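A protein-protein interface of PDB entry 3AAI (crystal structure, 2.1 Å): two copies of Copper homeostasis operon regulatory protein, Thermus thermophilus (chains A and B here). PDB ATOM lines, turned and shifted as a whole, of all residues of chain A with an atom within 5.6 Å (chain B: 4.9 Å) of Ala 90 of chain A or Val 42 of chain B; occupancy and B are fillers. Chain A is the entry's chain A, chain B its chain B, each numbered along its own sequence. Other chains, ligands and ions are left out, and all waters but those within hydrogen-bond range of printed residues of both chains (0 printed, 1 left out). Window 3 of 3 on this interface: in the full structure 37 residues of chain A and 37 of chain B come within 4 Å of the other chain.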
ATOM      1  N   HIS A  66      34.541 -30.138  15.303  1.00  0.00           N
ATOM      2  CA  HIS A  66      34.574 -28.978  16.186  1.00  0.00           C
ATOM      3  C   HIS A  66      34.988 -29.426  17.591  1.00  0.00           C
ATOM      4  O   HIS A  66      35.811 -28.779  18.239  1.00  0.00           O
ATOM      5  CB  HIS A  66      33.184 -28.327  16.223  1.00  0.00           C
ATOM      6  CG  HIS A  66      33.110 -27.067  17.032  1.00  0.00           C
ATOM      7  ND1 HIS A  66      33.726 -25.894  16.650  1.00  0.00           N
ATOM      8  CD2 HIS A  66      32.451 -26.785  18.181  1.00  0.00           C
ATOM      9  CE1 HIS A  66      33.447 -24.945  17.527  1.00  0.00           C
ATOM     10  NE2 HIS A  66      32.675 -25.460  18.466  1.00  0.00           N
ATOM     11  N   GLU A  85      29.377 -21.314  25.163  1.00  0.00           N
ATOM     12  CA  GLU A  85      28.215 -20.448  24.981  1.00  0.00           C
ATOM     13  C   GLU A  85      27.737 -20.463  23.534  1.00  0.00           C
ATOM     14  O   GLU A  85      26.543 -20.602  23.265  1.00  0.00           O
ATOM     15  CB  GLU A  85      28.556 -19.009  25.403  1.00  0.00           C
ATOM     16  N   GLU A  86      28.674 -20.320  22.602  1.00  0.00           N
ATOM     17  CA  GLU A  86      28.341 -20.308  21.181  1.00  0.00           C
ATOM     18  C   GLU A  86      27.789 -21.661  20.736  1.00  0.00           C
ATOM     19  O   GLU A  86      26.755 -21.731  20.069  1.00  0.00           O
ATOM     20  CB  GLU A  86      29.576 -19.942  20.358  1.00  0.00           C
ATOM     21  N   LEU A  87      28.482 -22.731  21.116  1.00  0.00           N
ATOM     22  CA  LEU A  87      28.061 -24.080  20.761  1.00  0.00           C
ATOM     23  C   LEU A  87      26.628 -24.363  21.206  1.00  0.00           C
ATOM     24  O   LEU A  87      25.779 -24.724  20.389  1.00  0.00           O
ATOM     25  CB  LEU A  87      28.999 -25.107  21.392  1.00  0.00           C
ATOM     26  CG  LEU A  87      28.689 -26.571  21.069  1.00  0.00           C
ATOM     27  CD1 LEU A  87      28.670 -26.777  19.556  1.00  0.00           C
ATOM     28  CD2 LEU A  87      29.738 -27.460  21.715  1.00  0.00           C
ATOM     29  N   MET A  88      26.365 -24.200  22.502  1.00  0.00           N
ATOM     30  CA  MET A  88      25.037 -24.436  23.054  1.00  0.00           C
ATOM     31  C   MET A  88      24.021 -23.589  22.299  1.00  0.00           C
ATOM     32  O   MET A  88      22.869 -23.989  22.112  1.00  0.00           O
ATOM     33  CB  MET A  88      25.001 -24.077  24.545  1.00  0.00           C
ATOM     34  CG  MET A  88      25.928 -24.906  25.423  1.00  0.00           C
ATOM     35  SD  MET A  88      25.506 -26.808  25.431  1.00  0.00           S
ATOM     36  CE  MET A  88      24.019 -26.765  26.673  1.00  0.00           C
ATOM     37  N   GLU A  89      24.464 -22.416  21.862  1.00  0.00           N
ATOM     38  CA  GLU A  89      23.617 -21.501  21.115  1.00  0.00           C
ATOM     39  C   GLU A  89      23.282 -22.119  19.757  1.00  0.00           C
ATOM     40  O   GLU A  89      22.150 -22.028  19.277  1.00  0.00           O
ATOM     41  CB  GLU A  89      24.350 -20.175  20.928  1.00  0.00           C
ATOM     42  CG  GLU A  89      23.497 -19.051  20.401  1.00  0.00           C
ATOM     43  CD  GLU A  89      24.241 -17.733  20.399  1.00  0.00           C
ATOM     44  OE1 GLU A  89      24.678 -17.300  21.486  1.00  0.00           O
ATOM     45  OE2 GLU A  89      24.392 -17.132  19.317  1.00  0.00           O
ATOM     46  N   ALA A  90      24.277 -22.754  19.145  1.00  0.00           N
ATOM     47  CA  ALA A  90      24.089 -23.396  17.852  1.00  0.00           C
ATOM     48  C   ALA A  90      23.232 -24.638  18.047  1.00  0.00           C
ATOM     49  O   ALA A  90      22.253 -24.846  17.335  1.00  0.00           O
ATOM     50  CB  ALA A  90      25.437 -23.776  17.249  1.00  0.00           C
ATOM     51  N   LEU A  91      23.608 -25.464  19.019  1.00  0.00           N
ATOM     52  CA  LEU A  91      22.857 -26.675  19.313  1.00  0.00           C
ATOM     53  C   LEU A  91      21.460 -26.232  19.731  1.00  0.00           C
ATOM     54  O   LEU A  91      20.490 -26.978  19.603  1.00  0.00           O
ATOM     55  CB  LEU A  91      23.536 -27.464  20.439  1.00  0.00           C
ATOM     56  CG  LEU A  91      24.966 -27.956  20.170  1.00  0.00           C
ATOM     57  CD1 LEU A  91      25.489 -28.708  21.383  1.00  0.00           C
ATOM     58  CD2 LEU A  91      24.983 -28.862  18.947  1.00  0.00           C
ATOM     59  N   LYS A  92      21.380 -24.998  20.218  1.00  0.00           N
ATOM     60  CA  LYS A  92      20.129 -24.389  20.652  1.00  0.00           C
ATOM     61  C   LYS A  92      19.485 -25.130  21.816  1.00  0.00           C
ATOM     62  O   LYS A  92      19.370 -24.517  22.899  1.00  0.00           O
ATOM     63  CB  LYS A  92      19.158 -24.308  19.468  1.00  0.00           C
ATOM     64  CG  LYS A  92      19.745 -23.578  18.263  1.00  0.00           C
ATOM     65  CD  LYS A  92      18.766 -23.467  17.105  1.00  0.00           C
ATOM     66  CE  LYS A  92      19.401 -22.722  15.937  1.00  0.00           C
ATOM     67  NZ  LYS A  92      18.457 -22.528  14.800  1.00  0.00           N
ATOM     68  N   TYR B  40      32.585 -20.554  10.029  1.00  0.00           N
ATOM     69  CA  TYR B  40      32.612 -21.056  11.401  1.00  0.00           C
ATOM     70  C   TYR B  40      31.685 -22.252  11.585  1.00  0.00           C
ATOM     71  O   TYR B  40      30.579 -22.285  11.047  1.00  0.00           O
ATOM     72  CB  TYR B  40      32.212 -19.960  12.394  1.00  0.00           C
ATOM     73  CG  TYR B  40      33.095 -18.729  12.379  1.00  0.00           C
ATOM     74  CD1 TYR B  40      34.482 -18.839  12.284  1.00  0.00           C
ATOM     75  CD2 TYR B  40      32.540 -17.453  12.492  1.00  0.00           C
ATOM     76  CE1 TYR B  40      35.298 -17.704  12.302  1.00  0.00           C
ATOM     77  CE2 TYR B  40      33.346 -16.314  12.513  1.00  0.00           C
ATOM     78  CZ  TYR B  40      34.723 -16.446  12.417  1.00  0.00           C
ATOM     79  OH  TYR B  40      35.520 -15.324  12.428  1.00  0.00           O
ATOM     80  N   CYS B  41      32.139 -23.225  12.368  1.00  0.00           N
ATOM     81  CA  CYS B  41      31.366 -24.433  12.620  1.00  0.00           C
ATOM     82  C   CYS B  41      29.955 -24.137  13.125  1.00  0.00           C
ATOM     83  O   CYS B  41      28.980 -24.691  12.617  1.00  0.00           O
ATOM     84  CB  CYS B  41      32.109 -25.322  13.625  1.00  0.00           C
ATOM     85  SG  CYS B  41      33.756 -25.869  13.071  1.00  0.00           S
ATOM     86  N   VAL B  42      29.852 -23.252  14.113  1.00  0.00           N
ATOM     87  CA  VAL B  42      28.569 -22.878  14.703  1.00  0.00           C
ATOM     88  C   VAL B  42      27.572 -22.293  13.704  1.00  0.00           C
ATOM     89  O   VAL B  42      26.364 -22.520  13.819  1.00  0.00           O
ATOM     90  CB  VAL B  42      28.775 -21.864  15.855  1.00  0.00           C
ATOM     91  CG1 VAL B  42      27.439 -21.303  16.310  1.00  0.00           C
ATOM     92  CG2 VAL B  42      29.481 -22.541  17.011  1.00  0.00           C
ATOM     93  N   ASP B  43      28.066 -21.528  12.732  1.00  0.00           N
ATOM     94  CA  ASP B  43      27.180 -20.934  11.732  1.00  0.00           C
ATOM     95  C   ASP B  43      26.556 -22.021  10.865  1.00  0.00           C
ATOM     96  O   ASP B  43      25.368 -21.976  10.558  1.00  0.00           O
ATOM     97  CB  ASP B  43      27.940 -19.943  10.848  1.00  0.00           C
ATOM     98  CG  ASP B  43      28.289 -18.660  11.581  1.00  0.00           C
ATOM     99  OD1 ASP B  43      27.372 -18.044  12.167  1.00  0.00           O
ATOM    100  OD2 ASP B  43      29.476 -18.269  11.568  1.00  0.00           O
ATOM    101  N   VAL B  44      27.369 -22.992  10.468  1.00  0.00           N
ATOM    102  CA  VAL B  44      26.886 -24.098   9.659  1.00  0.00           C
ATOM    103  C   VAL B  44      25.810 -24.839  10.452  1.00  0.00           C
ATOM    104  O   VAL B  44      24.718 -25.088   9.947  1.00  0.00           O
ATOM    105  CB  VAL B  44      28.034 -25.069   9.315  1.00  0.00           C
ATOM    106  CG1 VAL B  44      27.508 -26.236   8.484  1.00  0.00           C
ATOM    107  CG2 VAL B  44      29.120 -24.326   8.556  1.00  0.00           C
ATOM    108  N   LEU B  45      26.111 -25.165  11.704  1.00  0.00           N
ATOM    109  CA  LEU B  45      25.154 -25.882  12.546  1.00  0.00           C
ATOM    110  C   LEU B  45      23.855 -25.110  12.721  1.00  0.00           C
ATOM    111  O   LEU B  45      22.770 -25.691  12.695  1.00  0.00           O
ATOM    112  CB  LEU B  45      25.765 -26.182  13.921  1.00  0.00           C
ATOM    113  CG  LEU B  45      27.024 -27.059  13.921  1.00  0.00           C
ATOM    114  CD1 LEU B  45      27.483 -27.306  15.353  1.00  0.00           C
ATOM    115  CD2 LEU B  45      26.729 -28.386  13.226  1.00  0.00           C
ATOM    116  N   LYS B  46      23.966 -23.798  12.899  1.00  0.00           N
ATOM    117  CA  LYS B  46      22.786 -22.966  13.083  1.00  0.00           C
ATOM    118  C   LYS B  46      21.923 -22.909  11.830  1.00  0.00           C
ATOM    119  O   LYS B  46      20.697 -23.035  11.892  1.00  0.00           O
ATOM    120  CB  LYS B  46      23.191 -21.537  13.467  1.00  0.00           C
ATOM    121  CG  LYS B  46      23.690 -21.372  14.886  1.00  0.00           C
ATOM    122  CD  LYS B  46      23.930 -19.900  15.187  1.00  0.00           C
ATOM    123  CE  LYS B  46      24.278 -19.680  16.647  1.00  0.00           C
ATOM    124  NZ  LYS B  46      24.398 -18.226  16.960  1.00  0.00           N
ATOM    125  N   LYS B  49      20.178 -26.097  11.155  1.00  0.00           N
ATOM    126  CA  LYS B  49      19.025 -26.200  12.040  1.00  0.00           C
ATOM    127  C   LYS B  49      17.852 -25.423  11.463  1.00  0.00           C
ATOM    128  O   LYS B  49      16.698 -25.814  11.629  1.00  0.00           O
ATOM    129  CB  LYS B  49      19.360 -25.658  13.435  1.00  0.00           C
ATOM    130  CG  LYS B  49      20.311 -26.526  14.241  1.00  0.00           C
ATOM    131  CD  LYS B  49      19.720 -27.906  14.492  1.00  0.00           C
ATOM    132  CE  LYS B  49      20.711 -28.813  15.203  1.00  0.00           C
ATOM    133  NZ  LYS B  49      20.232 -30.222  15.230  1.00  0.00           N
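A ring nitrogen (ND1) of His 66 of chain A sits close to the side-chain sulfur of Cys 41 of chain B (3.6 Å). OE2 of Glu 89 of chain A lies within salt-bridge range of NZ of Lys 46 of chain B (2.6 Å).
Glu 86 of chain A touches Val 42 of chain B (O to CG1, 3.8 Å). Val 42 of chain B touches Ala 90 of chain A. Lys 46 of chain B touches Ala 90 of chain A. NZ of Lys 92 of chain A touches O of Lys 46 of chain B (3.7 Å). Lys 92 of chain A touches Lys 49 of chain B (NZ to CB, 3.5 Å).
Of chain B, only Val 42 (3.3 Å) and Lys 46 (3.6 Å) come within 4 Å of Ala 90 of chain A. Of the printed residues of chain B, Lys 92 of chain A touches Lys 46 and Lys 49. Val 42 of chain B touches just these residues of chain A: Glu 86 (3.8 Å) and Ala 90 (3.3 Å). Val 44 of chain B touches none of the printed residues of chain A. Of the printed residues of chain A, Lys 49 of chain B touches Lys 92. The nearest residue of chain B that does not touch Ala 90 of chain A is Lys 49 of chain B (4.02 Å). The nearest residue of chain A that does not touch Val 42 of chain B is Leu 87 of chain A (4.2 Å).
Of the 9 printed residues of chain A, 5 touch a printed residue of chain B. Hydrophobic or aromatic side chains of chain A that line the printed part of chain B: His 66 and Ala 90. Hydrophobic or aromatic side chains of chain B that line the printed part of chain A: Val 42. Among the printed residues, Asp or Glu carboxylates within 4 Å of a Lys or Arg side-chain nitrogen of the other chain: Glu 89 of chain A with Lys 46 of chain B.
No position is printed for both chains. Of the 7 pairs that touch across the chains among the printed residues, none has its exchanged pair printed and touching as well.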
